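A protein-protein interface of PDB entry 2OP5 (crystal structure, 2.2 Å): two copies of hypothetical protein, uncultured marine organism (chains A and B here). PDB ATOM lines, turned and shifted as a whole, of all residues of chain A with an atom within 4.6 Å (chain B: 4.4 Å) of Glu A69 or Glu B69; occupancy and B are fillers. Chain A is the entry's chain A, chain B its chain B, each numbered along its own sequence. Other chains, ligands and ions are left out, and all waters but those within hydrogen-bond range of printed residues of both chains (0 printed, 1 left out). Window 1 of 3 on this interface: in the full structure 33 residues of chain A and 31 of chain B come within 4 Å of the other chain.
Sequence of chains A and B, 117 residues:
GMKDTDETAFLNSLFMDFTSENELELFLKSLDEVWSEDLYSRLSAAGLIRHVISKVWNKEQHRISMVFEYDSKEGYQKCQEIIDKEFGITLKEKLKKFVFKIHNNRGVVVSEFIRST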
ATOM      1  N   THR A   8       6.175  24.546  21.346  1.00  0.00           N
ATOM      2  CA  THR A   8       7.081  23.872  20.430  1.00  0.00           C
ATOM      3  C   THR A   8       8.443  23.768  21.093  1.00  0.00           C
ATOM      4  O   THR A   8       8.985  24.758  21.549  1.00  0.00           O
ATOM      5  CB  THR A   8       7.224  24.647  19.083  1.00  0.00           C
ATOM      6  OG1 THR A   8       5.960  24.729  18.434  1.00  0.00           O
ATOM      7  CG2 THR A   8       8.184  23.947  18.137  1.00  0.00           C
ATOM      8  N   PHE A  10      10.921  21.389  19.563  1.00  0.00           N
ATOM      9  CA  PHE A  10      11.790  21.042  18.452  1.00  0.00           C
ATOM     10  C   PHE A  10      11.151  21.483  17.149  1.00  0.00           C
ATOM     11  O   PHE A  10       9.939  21.405  17.007  1.00  0.00           O
ATOM     12  CB  PHE A  10      12.000  19.544  18.436  1.00  0.00           C
ATOM     13  CG  PHE A  10      13.160  19.101  17.604  1.00  0.00           C
ATOM     14  CD1 PHE A  10      14.455  19.253  18.077  1.00  0.00           C
ATOM     15  CD2 PHE A  10      12.964  18.464  16.386  1.00  0.00           C
ATOM     16  CE1 PHE A  10      15.527  18.804  17.339  1.00  0.00           C
ATOM     17  CE2 PHE A  10      14.059  18.012  15.636  1.00  0.00           C
ATOM     18  CZ  PHE A  10      15.327  18.178  16.119  1.00  0.00           C
ATOM     19  N   LEU A  11      11.986  21.890  16.195  1.00  0.00           N
ATOM     20  CA  LEU A  11      11.520  22.454  14.941  1.00  0.00           C
ATOM     21  C   LEU A  11      12.447  22.186  13.742  1.00  0.00           C
ATOM     22  O   LEU A  11      13.670  22.100  13.886  1.00  0.00           O
ATOM     23  CB  LEU A  11      11.381  23.972  15.181  1.00  0.00           C
ATOM     24  CG  LEU A  11      10.984  25.075  14.202  1.00  0.00           C
ATOM     25  CD1 LEU A  11      10.479  26.287  14.956  1.00  0.00           C
ATOM     26  CD2 LEU A  11      12.120  25.481  13.289  1.00  0.00           C
ATOM     27  N   GLY A  47       3.165  13.978  18.109  1.00  0.00           N
ATOM     28  CA  GLY A  47       3.967  15.126  18.485  1.00  0.00           C
ATOM     29  C   GLY A  47       4.030  16.269  17.491  1.00  0.00           C
ATOM     30  O   GLY A  47       4.626  17.306  17.802  1.00  0.00           O
ATOM     31  N   LEU A  48       3.477  16.102  16.284  1.00  0.00           N
ATOM     32  CA  LEU A  48       3.453  17.232  15.357  1.00  0.00           C
ATOM     33  C   LEU A  48       2.409  18.216  15.896  1.00  0.00           C
ATOM     34  O   LEU A  48       1.259  17.836  16.187  1.00  0.00           O
ATOM     35  CB  LEU A  48       3.114  16.814  13.923  1.00  0.00           C
ATOM     36  CG  LEU A  48       3.180  17.927  12.878  1.00  0.00           C
ATOM     37  CD1 LEU A  48       4.608  18.377  12.625  1.00  0.00           C
ATOM     38  CD2 LEU A  48       2.532  17.489  11.589  1.00  0.00           C
ATOM     39  N   ILE A  49       2.843  19.457  16.093  1.00  0.00           N
ATOM     40  CA  ILE A  49       1.982  20.546  16.537  1.00  0.00           C
ATOM     41  C   ILE A  49       1.511  21.376  15.363  1.00  0.00           C
ATOM     42  O   ILE A  49       0.341  21.712  15.267  1.00  0.00           O
ATOM     43  CB  ILE A  49       2.736  21.491  17.501  1.00  0.00           C
ATOM     44  CG1 ILE A  49       3.158  20.712  18.756  1.00  0.00           C
ATOM     45  CG2 ILE A  49       1.881  22.738  17.836  1.00  0.00           C
ATOM     46  CD1 ILE A  49       4.063  21.483  19.718  1.00  0.00           C
ATOM     47  N   ARG A  50       2.433  21.688  14.460  1.00  0.00           N
ATOM     48  CA  ARG A  50       2.145  22.574  13.354  1.00  0.00           C
ATOM     49  C   ARG A  50       3.012  22.256  12.135  1.00  0.00           C
ATOM     50  O   ARG A  50       4.136  21.780  12.273  1.00  0.00           O
ATOM     51  CB  ARG A  50       2.373  24.014  13.827  1.00  0.00           C
ATOM     52  CG  ARG A  50       1.901  25.111  12.877  1.00  0.00           C
ATOM     53  CD  ARG A  50       2.312  26.464  13.400  1.00  0.00           C
ATOM     54  NE  ARG A  50       1.556  26.828  14.606  1.00  0.00           N
ATOM     55  CZ  ARG A  50       0.573  27.728  14.659  1.00  0.00           C
ATOM     56  NH1 ARG A  50       0.191  28.423  13.579  1.00  0.00           N
ATOM     57  NH2 ARG A  50      -0.031  27.954  15.831  1.00  0.00           N
ATOM     58  N   VAL A  52       3.525  24.195   8.250  1.00  0.00           N
ATOM     59  CA  VAL A  52       3.218  25.331   7.392  1.00  0.00           C
ATOM     60  C   VAL A  52       4.020  25.226   6.109  1.00  0.00           C
ATOM     61  O   VAL A  52       5.247  25.016   6.130  1.00  0.00           O
ATOM     62  CB  VAL A  52       3.607  26.657   8.067  1.00  0.00           C
ATOM     63  CG1 VAL A  52       2.927  27.829   7.352  1.00  0.00           C
ATOM     64  CG2 VAL A  52       3.220  26.643   9.531  1.00  0.00           C
ATOM     65  N   VAL A  67       7.840  24.491   7.545  1.00  0.00           N
ATOM     66  CA  VAL A  67       8.227  24.581   8.929  1.00  0.00           C
ATOM     67  C   VAL A  67       7.376  23.536   9.649  1.00  0.00           C
ATOM     68  O   VAL A  67       6.133  23.587   9.587  1.00  0.00           O
ATOM     69  CB  VAL A  67       7.991  25.986   9.531  1.00  0.00           C
ATOM     70  CG1 VAL A  67       8.363  25.985  11.003  1.00  0.00           C
ATOM     71  CG2 VAL A  67       8.768  27.080   8.764  1.00  0.00           C
ATOM     72  N   PHE A  68       8.053  22.570  10.273  1.00  0.00           N
ATOM     73  CA  PHE A  68       7.399  21.522  11.052  1.00  0.00           C
ATOM     74  C   PHE A  68       7.769  21.818  12.487  1.00  0.00           C
ATOM     75  O   PHE A  68       8.964  21.955  12.807  1.00  0.00           O
ATOM     76  CB  PHE A  68       7.964  20.120  10.771  1.00  0.00           C
ATOM     77  CG  PHE A  68       7.776  19.613   9.359  1.00  0.00           C
ATOM     78  CD1 PHE A  68       8.607  20.048   8.338  1.00  0.00           C
ATOM     79  CD2 PHE A  68       6.825  18.649   9.085  1.00  0.00           C
ATOM     80  CE1 PHE A  68       8.460  19.548   7.037  1.00  0.00           C
ATOM     81  CE2 PHE A  68       6.665  18.141   7.796  1.00  0.00           C
ATOM     82  CZ  PHE A  68       7.487  18.585   6.765  1.00  0.00           C
ATOM     83  N   GLU A  69       6.763  21.840  13.354  1.00  0.00           N
ATOM     84  CA  GLU A  69       6.965  22.098  14.770  1.00  0.00           C
ATOM     85  C   GLU A  69       6.453  20.931  15.606  1.00  0.00           C
ATOM     86  O   GLU A  69       5.330  20.450  15.408  1.00  0.00           O
ATOM     87  CB  GLU A  69       6.249  23.379  15.161  1.00  0.00           C
ATOM     88  CG  GLU A  69       6.776  24.577  14.397  1.00  0.00           C
ATOM     89  CD  GLU A  69       6.176  25.861  14.866  1.00  0.00           C
ATOM     90  OE1 GLU A  69       5.867  25.974  16.064  1.00  0.00           O
ATOM     91  OE2 GLU A  69       6.042  26.773  14.040  1.00  0.00           O
ATOM     92  N   TYR A  70       7.287  20.510  16.557  1.00  0.00           N
ATOM     93  CA  TYR A  70       6.987  19.380  17.395  1.00  0.00           C
ATOM     94  C   TYR A  70       7.068  19.734  18.857  1.00  0.00           C
ATOM     95  O   TYR A  70       7.837  20.608  19.249  1.00  0.00           O
ATOM     96  CB  TYR A  70       7.969  18.230  17.116  1.00  0.00           C
ATOM     97  CG  TYR A  70       8.122  17.853  15.650  1.00  0.00           C
ATOM     98  CD1 TYR A  70       9.062  18.483  14.859  1.00  0.00           C
ATOM     99  CD2 TYR A  70       7.324  16.866  15.063  1.00  0.00           C
ATOM    100  CE1 TYR A  70       9.216  18.161  13.523  1.00  0.00           C
ATOM    101  CE2 TYR A  70       7.474  16.519  13.698  1.00  0.00           C
ATOM    102  CZ  TYR A  70       8.418  17.182  12.940  1.00  0.00           C
ATOM    103  OH  TYR A  70       8.622  16.874  11.602  1.00  0.00           O
ATOM    104  N   ASP A  71       6.276  19.008  19.660  1.00  0.00           N
ATOM    105  CA  ASP A  71       6.274  19.145  21.112  1.00  0.00           C
ATOM    106  C   ASP A  71       7.616  18.680  21.710  1.00  0.00           C
ATOM    107  O   ASP A  71       7.951  19.064  22.825  1.00  0.00           O
ATOM    108  CB  ASP A  71       5.089  18.366  21.735  1.00  0.00           C
ATOM    109  CG  ASP A  71       5.142  16.856  21.473  1.00  0.00           C
ATOM    110  OD1 ASP A  71       6.154  16.326  20.979  1.00  0.00           O
ATOM    111  OD2 ASP A  71       4.163  16.169  21.795  1.00  0.00           O
ATOM    112  N   PHE B  10       0.999  34.790   5.852  1.00  0.00           N
ATOM    113  CA  PHE B  10       2.347  35.144   5.405  1.00  0.00           C
ATOM    114  C   PHE B  10       3.342  34.650   6.441  1.00  0.00           C
ATOM    115  O   PHE B  10       3.011  34.534   7.620  1.00  0.00           O
ATOM    116  CB  PHE B  10       2.450  36.666   5.215  1.00  0.00           C
ATOM    117  CG  PHE B  10       3.609  37.115   4.347  1.00  0.00           C
ATOM    118  CD1 PHE B  10       3.437  37.290   2.978  1.00  0.00           C
ATOM    119  CD2 PHE B  10       4.854  37.390   4.899  1.00  0.00           C
ATOM    120  CE1 PHE B  10       4.484  37.713   2.171  1.00  0.00           C
ATOM    121  CE2 PHE B  10       5.905  37.813   4.098  1.00  0.00           C
ATOM    122  CZ  PHE B  10       5.714  37.974   2.727  1.00  0.00           C
ATOM    123  N   LEU B  11       4.562  34.361   6.000  1.00  0.00           N
ATOM    124  CA  LEU B  11       5.568  33.823   6.901  1.00  0.00           C
ATOM    125  C   LEU B  11       6.982  34.106   6.454  1.00  0.00           C
ATOM    126  O   LEU B  11       7.305  33.860   5.308  1.00  0.00           O
ATOM    127  CB  LEU B  11       5.331  32.310   6.974  1.00  0.00           C
ATOM    128  CG  LEU B  11       6.122  31.383   7.906  1.00  0.00           C
ATOM    129  CD1 LEU B  11       5.274  30.197   8.292  1.00  0.00           C
ATOM    130  CD2 LEU B  11       7.408  30.880   7.306  1.00  0.00           C
ATOM    131  N   GLY B  47      -0.036  42.979  13.706  1.00  0.00           N
ATOM    132  CA  GLY B  47      -0.268  41.760  12.884  1.00  0.00           C
ATOM    133  C   GLY B  47       0.524  40.488  13.167  1.00  0.00           C
ATOM    134  O   GLY B  47       0.211  39.423  12.600  1.00  0.00           O
ATOM    135  N   LEU B  48       1.546  40.574  14.023  1.00  0.00           N
ATOM    136  CA  LEU B  48       2.396  39.421  14.339  1.00  0.00           C
ATOM    137  C   LEU B  48       1.645  38.397  15.181  1.00  0.00           C
ATOM    138  O   LEU B  48       1.156  38.711  16.261  1.00  0.00           O
ATOM    139  CB  LEU B  48       3.654  39.873  15.082  1.00  0.00           C
ATOM    140  CG  LEU B  48       4.686  38.815  15.491  1.00  0.00           C
ATOM    141  CD1 LEU B  48       5.300  38.144  14.275  1.00  0.00           C
ATOM    142  CD2 LEU B  48       5.771  39.428  16.353  1.00  0.00           C
ATOM    143  N   ILE B  49       1.583  37.163  14.681  1.00  0.00           N
ATOM    144  CA  ILE B  49       0.880  36.080  15.353  1.00  0.00           C
ATOM    145  C   ILE B  49       1.832  35.294  16.266  1.00  0.00           C
ATOM    146  O   ILE B  49       1.534  35.069  17.442  1.00  0.00           O
ATOM    147  CB  ILE B  49       0.285  35.066  14.334  1.00  0.00           C
ATOM    148  CG1 ILE B  49      -0.526  35.752  13.238  1.00  0.00           C
ATOM    149  CG2 ILE B  49      -0.588  34.055  15.031  1.00  0.00           C
ATOM    150  CD1 ILE B  49      -1.719  36.414  13.716  1.00  0.00           C
ATOM    151  N   ARG B  50       2.970  34.892  15.697  1.00  0.00           N
ATOM    152  CA  ARG B  50       3.950  34.051  16.368  1.00  0.00           C
ATOM    153  C   ARG B  50       5.350  34.406  15.951  1.00  0.00           C
ATOM    154  O   ARG B  50       5.580  34.946  14.869  1.00  0.00           O
ATOM    155  CB  ARG B  50       3.783  32.569  15.972  1.00  0.00           C
ATOM    156  CG  ARG B  50       2.461  31.970  16.319  1.00  0.00           C
ATOM    157  CD  ARG B  50       2.251  30.558  15.755  1.00  0.00           C
ATOM    158  NE  ARG B  50       2.775  29.539  16.661  1.00  0.00           N
ATOM    159  CZ  ARG B  50       3.937  28.888  16.536  1.00  0.00           C
ATOM    160  NH1 ARG B  50       4.758  29.083  15.498  1.00  0.00           N
ATOM    161  NH2 ARG B  50       4.253  27.993  17.461  1.00  0.00           N
ATOM    162  N   VAL B  52       9.132  32.250  16.640  1.00  0.00           N
ATOM    163  CA  VAL B  52       9.877  31.138  17.195  1.00  0.00           C
ATOM    164  C   VAL B  52      11.330  31.319  16.799  1.00  0.00           C
ATOM    165  O   VAL B  52      11.658  31.643  15.637  1.00  0.00           O
ATOM    166  CB  VAL B  52       9.387  29.789  16.660  1.00  0.00           C
ATOM    167  CG1 VAL B  52       9.858  28.654  17.577  1.00  0.00           C
ATOM    168  CG2 VAL B  52       7.878  29.778  16.573  1.00  0.00           C
ATOM    169  N   VAL B  67      11.302  32.006  12.725  1.00  0.00           N
ATOM    170  CA  VAL B  67      10.073  31.889  11.941  1.00  0.00           C
ATOM    171  C   VAL B  67       9.054  32.905  12.480  1.00  0.00           C
ATOM    172  O   VAL B  67       8.686  32.878  13.660  1.00  0.00           O
ATOM    173  CB  VAL B  67       9.469  30.484  12.032  1.00  0.00           C
ATOM    174  CG1 VAL B  67       8.186  30.418  11.217  1.00  0.00           C
ATOM    175  CG2 VAL B  67      10.459  29.460  11.546  1.00  0.00           C
ATOM    176  N   PHE B  68       8.635  33.816  11.603  1.00  0.00           N
ATOM    177  CA  PHE B  68       7.629  34.820  11.931  1.00  0.00           C
ATOM    178  C   PHE B  68       6.352  34.468  11.169  1.00  0.00           C
ATOM    179  O   PHE B  68       6.440  34.076  10.008  1.00  0.00           O
ATOM    180  CB  PHE B  68       8.067  36.205  11.470  1.00  0.00           C
ATOM    181  CG  PHE B  68       9.303  36.724  12.124  1.00  0.00           C
ATOM    182  CD1 PHE B  68      10.554  36.354  11.667  1.00  0.00           C
ATOM    183  CD2 PHE B  68       9.219  37.663  13.148  1.00  0.00           C
ATOM    184  CE1 PHE B  68      11.717  36.871  12.264  1.00  0.00           C
ATOM    185  CE2 PHE B  68      10.365  38.175  13.743  1.00  0.00           C
ATOM    186  CZ  PHE B  68      11.616  37.780  13.294  1.00  0.00           C
ATOM    187  N   GLU B  69       5.188  34.602  11.814  1.00  0.00           N
ATOM    188  CA  GLU B  69       3.879  34.352  11.179  1.00  0.00           C
ATOM    189  C   GLU B  69       2.978  35.571  11.353  1.00  0.00           C
ATOM    190  O   GLU B  69       2.812  36.086  12.461  1.00  0.00           O
ATOM    191  CB  GLU B  69       3.192  33.098  11.730  1.00  0.00           C
ATOM    192  CG  GLU B  69       3.923  31.786  11.386  1.00  0.00           C
ATOM    193  CD  GLU B  69       3.193  30.531  11.859  1.00  0.00           C
ATOM    194  OE1 GLU B  69       1.993  30.372  11.519  1.00  0.00           O
ATOM    195  OE2 GLU B  69       3.842  29.675  12.523  1.00  0.00           O
ATOM    196  N   TYR B  70       2.411  36.017  10.235  1.00  0.00           N
ATOM    197  CA  TYR B  70       1.543  37.174  10.189  1.00  0.00           C
ATOM    198  C   TYR B  70       0.152  36.748   9.744  1.00  0.00           C
ATOM    199  O   TYR B  70       0.003  35.764   9.015  1.00  0.00           O
ATOM    200  CB  TYR B  70       2.142  38.188   9.225  1.00  0.00           C
ATOM    201  CG  TYR B  70       3.598  38.486   9.552  1.00  0.00           C
ATOM    202  CD1 TYR B  70       3.931  39.418  10.532  1.00  0.00           C
ATOM    203  CD2 TYR B  70       4.633  37.822   8.910  1.00  0.00           C
ATOM    204  CE1 TYR B  70       5.246  39.691  10.850  1.00  0.00           C
ATOM    205  CE2 TYR B  70       5.963  38.095   9.219  1.00  0.00           C
ATOM    206  CZ  TYR B  70       6.257  39.035  10.193  1.00  0.00           C
ATOM    207  OH  TYR B  70       7.560  39.323  10.523  1.00  0.00           O
ATOM    208  N   GLU B 112      -1.588  25.049   5.806  1.00  0.00           N
ATOM    209  CA  GLU B 112      -1.177  25.030   7.190  1.00  0.00           C
ATOM    210  C   GLU B 112      -1.934  23.975   8.016  1.00  0.00           C
ATOM    211  O   GLU B 112      -3.149  23.798   7.866  1.00  0.00           O
ATOM    212  CB  GLU B 112      -1.394  26.431   7.773  1.00  0.00           C
ATOM    213  CG  GLU B 112      -1.017  26.579   9.228  1.00  0.00           C
ATOM    214  CD  GLU B 112      -1.112  28.011   9.728  1.00  0.00           C
ATOM    215  OE1 GLU B 112      -2.083  28.718   9.374  1.00  0.00           O
ATOM    216  OE2 GLU B 112      -0.218  28.415  10.500  1.00  0.00           O
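Of the 13 printed residues of chain A, 5 touch a printed residue of chain B.
Among the printed residues, Asp or Glu carboxylates within 4 Å of a Lys or Arg side-chain nitrogen of the other chain: Arg A50 with Glu B69 (3.4 Å), Arg A50 with Glu B112 (3.1 Å) and Glu A69 with Arg B50 (2.9 Å).
Of the printed residues of chain B, Glu A69 touches Arg B50 and Glu B69.
Of chain A, only Arg A50 (3.4 Å) and Glu A69 (3.9 Å) come within 4 Å of Glu B69.
Of the printed residues of chain B, Leu A11 touches Val B52 (3.6 Å).
Printed residues of chain A within 4 Å of Leu B11: Val A52 (3.5 Å).
Of the printed residues of chain B, Val A52 touches Leu B11 and Glu B112.
The nearest residue of chain B that does not touch Glu A69 is Val B52 (4.3 Å).
The nearest residue of chain A that does not touch Glu B69 is Val A52 (4.3 Å).
NE of Arg B50 lies close to NH2 of Arg A50, 3.3 Å away.
NH2 of Arg B50 lies within salt-bridge range of OE1 of Glu A69, 2.9 Å away.
NH1 of Arg A50 lies within salt-bridge range of OE1 of Glu B69.
The guanidinium group of Arg A50 is in salt-bridge range of the side-chain carboxylate of Glu B112, at 3.1 Å.
Arg B50 touches Thr A8 (NH2 to OG1, 3.8 Å).
CG1 of Val B52 touches CD1 of Leu A11, at 3.6 Å.
Val A52 touches Leu B11 (CG1 to CD1, 3.5 Å).
CG2 of Val A52 touches OE2 of Glu B112 (3.99 Å).
OE2 of Glu A69 touches OE2 of Glu B69 (3.9 Å).
Leu A11 touches Val B52, and with the chains exchanged Val A52 touches Leu B11.
Arg B50 touches its own counterpart, Arg A50.
Arg A50 touches Glu B69, and with the chains exchanged Glu A69 touches Arg B50.
Glu B69 touches its own counterpart, Glu A69.
O of Val A67 is in hydrogen-bond range of N of Val A52, 3.0 Å away.
N of Ile B49 sits at hydrogen-bond distance from O of Glu B69 (2.8 Å).
O of Arg A50 lies within hydrogen-bond range of N of Glu A69 (2.8 Å).
The backbone NH (N) of Ile A49 sits at hydrogen-bond distance from the backbone carbonyl oxygen (O) of Glu A69, 2.8 Å away.
N of Val B67 is in hydrogen-bond range of O of Val B52 (3.0 Å).
The side-chain carboxylate (OE1) of Glu A69 lies within hydrogen-bond range of the side-chain hydroxyl (OG1) of Thr A8, 2.7 Å away.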
